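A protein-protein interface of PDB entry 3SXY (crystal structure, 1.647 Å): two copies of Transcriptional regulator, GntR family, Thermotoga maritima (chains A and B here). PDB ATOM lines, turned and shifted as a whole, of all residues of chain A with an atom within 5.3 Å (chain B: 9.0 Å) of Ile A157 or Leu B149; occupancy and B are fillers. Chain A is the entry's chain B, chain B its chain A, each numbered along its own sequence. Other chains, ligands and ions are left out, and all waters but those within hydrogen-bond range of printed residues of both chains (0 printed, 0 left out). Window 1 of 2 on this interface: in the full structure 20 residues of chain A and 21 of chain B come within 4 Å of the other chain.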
ATOM      1  N   GLU A  85      11.644  -3.251  -7.158  1.00  0.00           N
ATOM      2  CA  GLU A  85      12.471  -3.998  -8.104  1.00  0.00           C
ATOM      3  C   GLU A  85      12.798  -5.361  -7.588  1.00  0.00           C
ATOM      4  O   GLU A  85      12.764  -6.340  -8.371  1.00  0.00           O
ATOM      5  CB  GLU A  85      13.689  -3.192  -8.556  1.00  0.00           C
ATOM      6  CG  GLU A  85      13.247  -1.963  -9.401  1.00  0.00           C
ATOM      7  CD  GLU A  85      14.383  -1.229 -10.094  1.00  0.00           C
ATOM      8  OE1 GLU A  85      15.551  -1.538  -9.740  1.00  0.00           O
ATOM      9  OE2 GLU A  85      14.118  -0.280 -10.921  1.00  0.00           O
ATOM     10  N   THR A  86      13.105  -5.512  -6.284  1.00  0.00           N
ATOM     11  CA  THR A  86      13.287  -6.833  -5.725  1.00  0.00           C
ATOM     12  C   THR A  86      12.057  -7.735  -5.875  1.00  0.00           C
ATOM     13  O   THR A  86      12.154  -8.915  -6.279  1.00  0.00           O
ATOM     14  CB  THR A  86      13.612  -6.747  -4.213  1.00  0.00           C
ATOM     15  OG1 THR A  86      14.744  -5.932  -4.054  1.00  0.00           O
ATOM     16  CG2 THR A  86      13.918  -8.134  -3.687  1.00  0.00           C
ATOM     17  N   THR A  89      11.365  -8.979  -9.387  1.00  0.00           N
ATOM     18  CA  THR A  89      12.328  -9.993  -9.724  1.00  0.00           C
ATOM     19  C   THR A  89      11.978 -11.318  -9.057  1.00  0.00           C
ATOM     20  O   THR A  89      12.091 -12.412  -9.683  1.00  0.00           O
ATOM     21  CB  THR A  89      13.783  -9.513  -9.408  1.00  0.00           C
ATOM     22  OG1 THR A  89      14.076  -8.291 -10.065  1.00  0.00           O
ATOM     23  CG2 THR A  89      14.777 -10.540  -9.838  1.00  0.00           C
ATOM     24  N   ARG A  90      11.532 -11.291  -7.790  1.00  0.00           N
ATOM     25  CA  ARG A  90      11.025 -12.482  -7.137  1.00  0.00           C
ATOM     26  C   ARG A  90       9.852 -13.090  -7.847  1.00  0.00           C
ATOM     27  O   ARG A  90       9.795 -14.299  -8.026  1.00  0.00           O
ATOM     28  CB  ARG A  90      10.613 -12.245  -5.680  1.00  0.00           C
ATOM     29  CG  ARG A  90      11.695 -12.003  -4.797  1.00  0.00           C
ATOM     30  CD  ARG A  90      11.129 -11.783  -3.392  1.00  0.00           C
ATOM     31  NE  ARG A  90      10.694 -13.012  -2.756  1.00  0.00           N
ATOM     32  CZ  ARG A  90      10.179 -13.085  -1.531  1.00  0.00           C
ATOM     33  NH1 ARG A  90      10.121 -12.008  -0.745  1.00  0.00           N
ATOM     34  NH2 ARG A  90       9.795 -14.253  -1.090  1.00  0.00           N
ATOM     35  N   MET A  93      11.137 -14.841 -10.996  1.00  0.00           N
ATOM     36  CA  MET A  93      11.906 -16.061 -10.801  1.00  0.00           C
ATOM     37  C   MET A  93      11.129 -17.197 -10.116  1.00  0.00           C
ATOM     38  O   MET A  93      11.172 -18.343 -10.555  1.00  0.00           O
ATOM     39  CB  MET A  93      13.185 -15.724 -10.081  1.00  0.00           C
ATOM     40  CG  MET A  93      14.098 -14.676 -10.736  1.00  0.00           C
ATOM     41  SD  MET A  93      15.606 -14.237  -9.803  1.00  0.00           S
ATOM     42  CE  MET A  93      16.506 -15.744  -9.988  1.00  0.00           C
ATOM     43  N   LEU A 153      21.840 -16.409  -8.875  1.00  0.00           N
ATOM     44  CA  LEU A 153      21.238 -15.073  -8.968  1.00  0.00           C
ATOM     45  C   LEU A 153      20.244 -14.877  -7.818  1.00  0.00           C
ATOM     46  O   LEU A 153      20.245 -13.810  -7.207  1.00  0.00           O
ATOM     47  CB  LEU A 153      20.510 -14.872 -10.289  1.00  0.00           C
ATOM     48  CG  LEU A 153      21.361 -14.860 -11.540  1.00  0.00           C
ATOM     49  CD1 LEU A 153      20.444 -14.675 -12.695  1.00  0.00           C
ATOM     50  CD2 LEU A 153      22.483 -13.828 -11.570  1.00  0.00           C
ATOM     51  N   TYR A 154      19.428 -15.876  -7.541  1.00  0.00           N
ATOM     52  CA  TYR A 154      18.406 -15.773  -6.493  1.00  0.00           C
ATOM     53  C   TYR A 154      19.058 -15.636  -5.098  1.00  0.00           C
ATOM     54  O   TYR A 154      18.500 -14.970  -4.243  1.00  0.00           O
ATOM     55  CB  TYR A 154      17.464 -16.958  -6.538  1.00  0.00           C
ATOM     56  CG  TYR A 154      16.239 -16.685  -5.686  1.00  0.00           C
ATOM     57  CD1 TYR A 154      15.182 -15.950  -6.177  1.00  0.00           C
ATOM     58  CD2 TYR A 154      16.138 -17.199  -4.442  1.00  0.00           C
ATOM     59  CE1 TYR A 154      14.076 -15.670  -5.387  1.00  0.00           C
ATOM     60  CE2 TYR A 154      15.069 -16.937  -3.653  1.00  0.00           C
ATOM     61  CZ  TYR A 154      14.027 -16.213  -4.121  1.00  0.00           C
ATOM     62  OH  TYR A 154      12.965 -16.029  -3.276  1.00  0.00           O
ATOM     63  N   GLU A 155      20.247 -16.242  -4.885  1.00  0.00           N
ATOM     64  CA  GLU A 155      20.976 -16.024  -3.616  1.00  0.00           C
ATOM     65  C   GLU A 155      21.179 -14.536  -3.336  1.00  0.00           C
ATOM     66  O   GLU A 155      20.979 -14.083  -2.222  1.00  0.00           O
ATOM     67  CB  GLU A 155      22.318 -16.727  -3.517  1.00  0.00           C
ATOM     68  CG  GLU A 155      22.252 -18.219  -3.447  1.00  0.00           C
ATOM     69  CD  GLU A 155      21.743 -18.703  -2.108  1.00  0.00           C
ATOM     70  OE1 GLU A 155      22.442 -18.479  -1.094  1.00  0.00           O
ATOM     71  OE2 GLU A 155      20.661 -19.291  -2.081  1.00  0.00           O
ATOM     72  N   LYS A 156      21.555 -13.754  -4.355  1.00  0.00           N
ATOM     73  CA  LYS A 156      21.714 -12.326  -4.172  1.00  0.00           C
ATOM     74  C   LYS A 156      20.389 -11.589  -4.087  1.00  0.00           C
ATOM     75  O   LYS A 156      20.315 -10.583  -3.410  1.00  0.00           O
ATOM     76  CB  LYS A 156      22.600 -11.751  -5.273  1.00  0.00           C
ATOM     77  CG  LYS A 156      23.961 -12.382  -5.246  1.00  0.00           C
ATOM     78  CD  LYS A 156      24.860 -11.866  -6.294  1.00  0.00           C
ATOM     79  CE  LYS A 156      25.941 -12.863  -6.630  1.00  0.00           C
ATOM     80  NZ  LYS A 156      26.390 -12.722  -8.042  1.00  0.00           N
ATOM     81  N   ILE A 157      19.331 -12.051  -4.739  1.00  0.00           N
ATOM     82  CA  ILE A 157      18.044 -11.410  -4.588  1.00  0.00           C
ATOM     83  C   ILE A 157      17.571 -11.619  -3.163  1.00  0.00           C
ATOM     84  O   ILE A 157      17.035 -10.689  -2.558  1.00  0.00           O
ATOM     85  CB  ILE A 157      17.013 -12.005  -5.558  1.00  0.00           C
ATOM     86  CG1 ILE A 157      17.454 -11.755  -6.996  1.00  0.00           C
ATOM     87  CG2 ILE A 157      15.588 -11.584  -5.265  1.00  0.00           C
ATOM     88  CD1 ILE A 157      17.498 -10.356  -7.380  1.00  0.00           C
ATOM     89  N   TRP A 158      17.884 -12.792  -2.605  1.00  0.00           N
ATOM     90  CA  TRP A 158      17.448 -13.058  -1.194  1.00  0.00           C
ATOM     91  C   TRP A 158      18.214 -12.090  -0.221  1.00  0.00           C
ATOM     92  O   TRP A 158      17.713 -11.688   0.814  1.00  0.00           O
ATOM     93  CB  TRP A 158      17.606 -14.532  -0.733  1.00  0.00           C
ATOM     94  CG  TRP A 158      16.853 -14.720   0.556  1.00  0.00           C
ATOM     95  CD1 TRP A 158      17.357 -14.602   1.852  1.00  0.00           C
ATOM     96  CD2 TRP A 158      15.436 -14.928   0.688  1.00  0.00           C
ATOM     97  NE1 TRP A 158      16.329 -14.736   2.755  1.00  0.00           N
ATOM     98  CE2 TRP A 158      15.142 -14.912   2.075  1.00  0.00           C
ATOM     99  CE3 TRP A 158      14.371 -15.077  -0.221  1.00  0.00           C
ATOM    100  CZ2 TRP A 158      13.829 -15.065   2.546  1.00  0.00           C
ATOM    101  CZ3 TRP A 158      13.088 -15.251   0.262  1.00  0.00           C
ATOM    102  CH2 TRP A 158      12.839 -15.260   1.634  1.00  0.00           C
ATOM    103  N   ASP A 159      19.466 -11.726  -0.524  1.00  0.00           N
ATOM    104  CA  ASP A 159      20.198 -10.725   0.278  1.00  0.00           C
ATOM    105  C   ASP A 159      19.390  -9.404   0.367  1.00  0.00           C
ATOM    106  O   ASP A 159      19.352  -8.736   1.402  1.00  0.00           O
ATOM    107  CB  ASP A 159      21.566 -10.432  -0.299  1.00  0.00           C
ATOM    108  CG  ASP A 159      22.522 -11.602  -0.237  1.00  0.00           C
ATOM    109  OD1 ASP A 159      22.427 -12.447   0.682  1.00  0.00           O
ATOM    110  OD2 ASP A 159      23.485 -11.629  -1.084  1.00  0.00           O
ATOM    111  N   ARG A 160      18.771  -9.012  -0.743  1.00  0.00           N
ATOM    112  CA  ARG A 160      18.019  -7.753  -0.825  1.00  0.00           C
ATOM    113  C   ARG A 160      16.739  -7.868   0.013  1.00  0.00           C
ATOM    114  O   ARG A 160      16.311  -6.896   0.642  1.00  0.00           O
ATOM    115  CB  ARG A 160      17.643  -7.414  -2.272  1.00  0.00           C
ATOM    116  CG  ARG A 160      18.851  -7.148  -3.191  1.00  0.00           C
ATOM    117  CD  ARG A 160      18.386  -7.028  -4.624  1.00  0.00           C
ATOM    118  NE  ARG A 160      17.468  -5.880  -4.831  1.00  0.00           N
ATOM    119  CZ  ARG A 160      17.773  -4.717  -5.359  1.00  0.00           C
ATOM    120  NH1 ARG A 160      19.038  -4.409  -5.759  1.00  0.00           N
ATOM    121  NH2 ARG A 160      16.796  -3.804  -5.555  1.00  0.00           N
ATOM    122  N   ILE A 161      16.191  -9.063   0.066  1.00  0.00           N
ATOM    123  CA  ILE A 161      15.020  -9.376   0.917  1.00  0.00           C
ATOM    124  C   ILE A 161      15.413  -9.309   2.373  1.00  0.00           C
ATOM    125  O   ILE A 161      14.712  -8.705   3.209  1.00  0.00           O
ATOM    126  CB  ILE A 161      14.432 -10.762   0.563  1.00  0.00           C
ATOM    127  CG1 ILE A 161      13.862 -10.742  -0.856  1.00  0.00           C
ATOM    128  CG2 ILE A 161      13.344 -11.230   1.581  1.00  0.00           C
ATOM    129  CD1 ILE A 161      13.761 -12.237  -1.453  1.00  0.00           C
ATOM    130  N   MET B  92      13.066 -17.330 -19.074  1.00  0.00           N
ATOM    131  CA  MET B  92      12.426 -16.784 -17.870  1.00  0.00           C
ATOM    132  C   MET B  92      12.306 -15.256 -17.957  1.00  0.00           C
ATOM    133  O   MET B  92      11.219 -14.714 -17.713  1.00  0.00           O
ATOM    134  CB  MET B  92      13.256 -17.162 -16.607  1.00  0.00           C
ATOM    135  CG  MET B  92      12.804 -16.519 -15.292  1.00  0.00           C
ATOM    136  SD  MET B  92      13.838 -16.988 -13.929  1.00  0.00           S
ATOM    137  CE  MET B  92      15.379 -16.121 -14.300  1.00  0.00           C
ATOM    138  N   MET B  93      13.410 -14.568 -18.273  1.00  0.00           N
ATOM    139  CA  MET B  93      13.407 -13.122 -18.188  1.00  0.00           C
ATOM    140  C   MET B  93      12.667 -12.456 -19.349  1.00  0.00           C
ATOM    141  O   MET B  93      11.843 -11.524 -19.148  1.00  0.00           O
ATOM    142  CB  MET B  93      14.837 -12.605 -18.109  1.00  0.00           C
ATOM    143  CG  MET B  93      15.590 -13.088 -16.867  1.00  0.00           C
ATOM    144  SD  MET B  93      17.307 -12.559 -16.797  1.00  0.00           S
ATOM    145  CE  MET B  93      16.979 -10.838 -16.332  1.00  0.00           C
ATOM    146  N   ILE B 142      13.394  -6.439 -22.219  1.00  0.00           N
ATOM    147  CA  ILE B 142      13.835  -6.248 -20.830  1.00  0.00           C
ATOM    148  C   ILE B 142      13.725  -4.786 -20.418  1.00  0.00           C
ATOM    149  O   ILE B 142      13.205  -4.470 -19.293  1.00  0.00           O
ATOM    150  CB  ILE B 142      15.225  -6.766 -20.641  1.00  0.00           C
ATOM    151  CG1 ILE B 142      15.360  -8.237 -21.060  1.00  0.00           C
ATOM    152  CG2 ILE B 142      15.676  -6.534 -19.202  1.00  0.00           C
ATOM    153  CD1 ILE B 142      14.540  -9.198 -20.269  1.00  0.00           C
ATOM    154  N   SER B 145      10.468  -3.053 -19.055  1.00  0.00           N
ATOM    155  CA  SER B 145      10.033  -3.268 -17.661  1.00  0.00           C
ATOM    156  C   SER B 145      10.314  -2.023 -16.826  1.00  0.00           C
ATOM    157  O   SER B 145       9.654  -1.794 -15.779  1.00  0.00           O
ATOM    158  CB  SER B 145      10.726  -4.463 -17.032  1.00  0.00           C
ATOM    159  OG  SER B 145      12.133  -4.245 -16.829  1.00  0.00           O
ATOM    160  N   GLY B 146      11.304  -1.232 -17.222  1.00  0.00           N
ATOM    161  CA  GLY B 146      11.805  -0.147 -16.397  1.00  0.00           C
ATOM    162  C   GLY B 146      12.423  -0.572 -15.069  1.00  0.00           C
ATOM    163  O   GLY B 146      12.597   0.248 -14.154  1.00  0.00           O
ATOM    164  N   ASN B 147      12.739  -1.838 -14.941  1.00  0.00           N
ATOM    165  CA  ASN B 147      13.277  -2.412 -13.722  1.00  0.00           C
ATOM    166  C   ASN B 147      14.763  -2.454 -13.869  1.00  0.00           C
ATOM    167  O   ASN B 147      15.332  -3.301 -14.550  1.00  0.00           O
ATOM    168  CB  ASN B 147      12.647  -3.790 -13.455  1.00  0.00           C
ATOM    169  CG  ASN B 147      13.135  -4.448 -12.186  1.00  0.00           C
ATOM    170  OD1 ASN B 147      14.308  -4.410 -11.850  1.00  0.00           O
ATOM    171  ND2 ASN B 147      12.213  -5.076 -11.480  1.00  0.00           N
ATOM    172  N   GLU B 148      15.440  -1.531 -13.188  1.00  0.00           N
ATOM    173  CA  GLU B 148      16.879  -1.425 -13.330  1.00  0.00           C
ATOM    174  C   GLU B 148      17.649  -2.667 -12.868  1.00  0.00           C
ATOM    175  O   GLU B 148      18.707  -2.974 -13.395  1.00  0.00           O
ATOM    176  CB  GLU B 148      17.405  -0.187 -12.631  1.00  0.00           C
ATOM    177  CG  GLU B 148      16.959   1.162 -13.283  1.00  0.00           C
ATOM    178  CD  GLU B 148      17.265   1.281 -14.781  1.00  0.00           C
ATOM    179  OE1 GLU B 148      18.329   0.769 -15.240  1.00  0.00           O
ATOM    180  OE2 GLU B 148      16.445   1.911 -15.499  1.00  0.00           O
ATOM    181  N   LEU B 149      17.113  -3.388 -11.866  1.00  0.00           N
ATOM    182  CA  LEU B 149      17.713  -4.604 -11.364  1.00  0.00           C
ATOM    183  C   LEU B 149      17.651  -5.665 -12.472  1.00  0.00           C
ATOM    184  O   LEU B 149      18.682  -6.262 -12.769  1.00  0.00           O
ATOM    185  CB  LEU B 149      17.027  -5.128 -10.110  1.00  0.00           C
ATOM    186  CG  LEU B 149      17.504  -6.433  -9.508  1.00  0.00           C
ATOM    187  CD1 LEU B 149      18.997  -6.460  -9.234  1.00  0.00           C
ATOM    188  CD2 LEU B 149      16.659  -6.757  -8.264  1.00  0.00           C
ATOM    189  N   ILE B 150      16.492  -5.873 -13.084  1.00  0.00           N
ATOM    190  CA  ILE B 150      16.326  -6.884 -14.141  1.00  0.00           C
ATOM    191  C   ILE B 150      17.230  -6.463 -15.332  1.00  0.00           C
ATOM    192  O   ILE B 150      17.907  -7.329 -15.919  1.00  0.00           O
ATOM    193  CB  ILE B 150      14.871  -7.080 -14.525  1.00  0.00           C
ATOM    194  CG1 ILE B 150      14.150  -7.764 -13.340  1.00  0.00           C
ATOM    195  CG2 ILE B 150      14.757  -7.955 -15.782  1.00  0.00           C
ATOM    196  CD1 ILE B 150      12.645  -7.943 -13.556  1.00  0.00           C
ATOM    197  N   ILE B 151      17.198  -5.197 -15.695  1.00  0.00           N
ATOM    198  CA  ILE B 151      18.035  -4.700 -16.814  1.00  0.00           C
ATOM    199  C   ILE B 151      19.515  -4.993 -16.539  1.00  0.00           C
ATOM    200  O   ILE B 151      20.262  -5.491 -17.388  1.00  0.00           O
ATOM    201  CB  ILE B 151      17.755  -3.204 -17.087  1.00  0.00           C
ATOM    202  CG1 ILE B 151      16.323  -3.014 -17.621  1.00  0.00           C
ATOM    203  CG2 ILE B 151      18.847  -2.583 -17.953  1.00  0.00           C
ATOM    204  CD1 ILE B 151      15.848  -1.497 -17.585  1.00  0.00           C
ATOM    205  N   SER B 152      19.983  -4.730 -15.327  1.00  0.00           N
ATOM    206  CA  SER B 152      21.375  -4.976 -15.005  1.00  0.00           C
ATOM    207  C   SER B 152      21.734  -6.460 -15.002  1.00  0.00           C
ATOM    208  O   SER B 152      22.815  -6.868 -15.453  1.00  0.00           O
ATOM    209  CB  SER B 152      21.741  -4.281 -13.680  1.00  0.00           C
ATOM    210  OG  SER B 152      21.257  -4.961 -12.536  1.00  0.00           O
ATOM    211  N   LEU B 153      20.829  -7.320 -14.521  1.00  0.00           N
ATOM    212  CA  LEU B 153      21.068  -8.727 -14.541  1.00  0.00           C
ATOM    213  C   LEU B 153      21.138  -9.211 -15.984  1.00  0.00           C
ATOM    214  O   LEU B 153      22.003 -10.016 -16.319  1.00  0.00           O
ATOM    215  CB  LEU B 153      19.965  -9.477 -13.813  1.00  0.00           C
ATOM    216  CG  LEU B 153      19.875  -9.231 -12.299  1.00  0.00           C
ATOM    217  CD1 LEU B 153      18.709 -10.055 -11.816  1.00  0.00           C
ATOM    218  CD2 LEU B 153      21.135  -9.572 -11.517  1.00  0.00           C
ATOM    219  N   TYR B 154      20.259  -8.701 -16.846  1.00  0.00           N
ATOM    220  CA  TYR B 154      20.185  -9.210 -18.224  1.00  0.00           C
ATOM    221  C   TYR B 154      21.441  -8.739 -19.015  1.00  0.00           C
ATOM    222  O   TYR B 154      21.869  -9.440 -19.928  1.00  0.00           O
ATOM    223  CB  TYR B 154      18.935  -8.721 -18.929  1.00  0.00           C
ATOM    224  CG  TYR B 154      18.689  -9.444 -20.230  1.00  0.00           C
ATOM    225  CD1 TYR B 154      18.159 -10.672 -20.260  1.00  0.00           C
ATOM    226  CD2 TYR B 154      19.047  -8.821 -21.427  1.00  0.00           C
ATOM    227  CE1 TYR B 154      17.972 -11.326 -21.487  1.00  0.00           C
ATOM    228  CE2 TYR B 154      18.873  -9.419 -22.620  1.00  0.00           C
ATOM    229  CZ  TYR B 154      18.328 -10.650 -22.636  1.00  0.00           C
ATOM    230  OH  TYR B 154      18.158 -11.279 -23.864  1.00  0.00           O
ATOM    231  N   GLU B 155      22.036  -7.594 -18.668  1.00  0.00           N
ATOM    232  CA  GLU B 155      23.311  -7.139 -19.294  1.00  0.00           C
ATOM    233  C   GLU B 155      24.326  -8.237 -19.152  1.00  0.00           C
ATOM    234  O   GLU B 155      25.093  -8.528 -20.071  1.00  0.00           O
ATOM    235  CB  GLU B 155      23.865  -5.833 -18.670  1.00  0.00           C
ATOM    236  CG  GLU B 155      23.089  -4.600 -19.002  1.00  0.00           C
ATOM    237  CD  GLU B 155      23.199  -4.187 -20.463  1.00  0.00           C
ATOM    238  OE1 GLU B 155      24.283  -3.739 -20.888  1.00  0.00           O
ATOM    239  OE2 GLU B 155      22.194  -4.286 -21.174  1.00  0.00           O
ATOM    240  N   LYS B 156      24.388  -8.871 -18.001  1.00  0.00           N
ATOM    241  CA  LYS B 156      25.359  -9.934 -17.768  1.00  0.00           C
ATOM    242  C   LYS B 156      24.989 -11.239 -18.432  1.00  0.00           C
ATOM    243  O   LYS B 156      25.847 -11.973 -18.891  1.00  0.00           O
ATOM    244  CB  LYS B 156      25.657 -10.106 -16.279  1.00  0.00           C
ATOM    245  CG  LYS B 156      26.249  -8.844 -15.689  1.00  0.00           C
ATOM    246  CD  LYS B 156      26.482  -8.980 -14.202  1.00  0.00           C
ATOM    247  CE  LYS B 156      26.504  -7.614 -13.490  1.00  0.00           C
ATOM    248  NZ  LYS B 156      26.208  -7.704 -12.022  1.00  0.00           N
ATOM    249  N   ILE B 157      23.705 -11.559 -18.516  1.00  0.00           N
ATOM    250  CA  ILE B 157      23.238 -12.677 -19.266  1.00  0.00           C
ATOM    251  C   ILE B 157      23.623 -12.506 -20.746  1.00  0.00           C
ATOM    252  O   ILE B 157      24.065 -13.505 -21.377  1.00  0.00           O
ATOM    253  CB  ILE B 157      21.722 -12.842 -19.147  1.00  0.00           C
ATOM    254  CG1 ILE B 157      21.263 -13.144 -17.684  1.00  0.00           C
ATOM    255  CG2 ILE B 157      21.232 -13.973 -20.038  1.00  0.00           C
ATOM    256  CD1 ILE B 157      21.962 -14.276 -17.070  1.00  0.00           C
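N of Glu B148 sits at hydrogen-bond distance from OE2 of Glu A85 (2.9 Å).
OE1 of Glu A85 sits at hydrogen-bond distance from N of Leu B149 (3.2 Å).
The backbone carbonyl oxygen (O) of Glu A85 lies within hydrogen-bond range of the side-chain amide nitrogen (ND2) of Asn B147 (3.4 Å).
OG of Ser B145 sits close to N of Asn B147 (3.1 Å).
OD1 of Asn B147 is in hydrogen-bond range of N of Leu B149.
O of Leu B149 is in hydrogen-bond range of OG of Ser B152 (2.9 Å).
The side-chain hydroxyl (OG1) of Thr A86 is in hydrogen-bond range of the guanidinium group (NE) of Arg A160 (2.8 Å).
The backbone carbonyl oxygen (O) of Glu A85 sits at hydrogen-bond distance from the side-chain hydroxyl (OG1) of Thr A89, at 2.9 Å.
The side-chain amide oxygen (OD1) of Asn B147 lies within hydrogen-bond range of the backbone NH (N) of Ile B150 (2.9 Å).
Gly B146 touches Glu A85 (O to OE2, 3.6 Å).
Asn B147 touches Thr A89 (ND2 to OG1, 3.98 Å).
Leu B149 touches Thr A89 (CD2 to OG1, 3.5 Å).
Thr A89 touches Ile B150 (OG1 to CG1, 3.3 Å).
CA of Met A93 touches SD of Met B92, at 3.8 Å.
Leu B149 touches Ile A157 (CD2 to CD1, 3.8 Å).
Leu B149 touches Arg A160 (CD2 to NE, 3.6 Å).
Of the printed residues of chain B, Glu A85 touches Gly B146, Asn B147, Glu B148 and Leu B149.
Of the printed residues of chain B, Met A93 touches Met B92 (3.8 Å).
Ile A157 touches one residue of chain B.
Printed residues of chain A within 4 Å of Met B92: Met A93 (3.8 Å).
Leu B149 touches just these residues of chain A: Glu A85, Thr A89, Ile A157 and Arg A160.
The nearest residue of chain A that does not touch Leu B149 is Thr A86 (4.2 Å).
The nearest printed residue of chain A that does not touch Glu B148 is Thr A89 (7.2 Å).
Printed residues of chain B that touch a printed residue of chain A: Met B92, Gly B146, Asn B147, Glu B148, Leu B149 and Ile B150.
Of the 14 printed residues of chain A, 5 touch a printed residue of chain B.
Hydrophobic or aromatic side chains of chain A within 4 Å of the printed part of chain B: Met A93 and Ile A157.
Among the printed residues, 10 pairs touch across the chains.
6 positions are printed for both chains.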
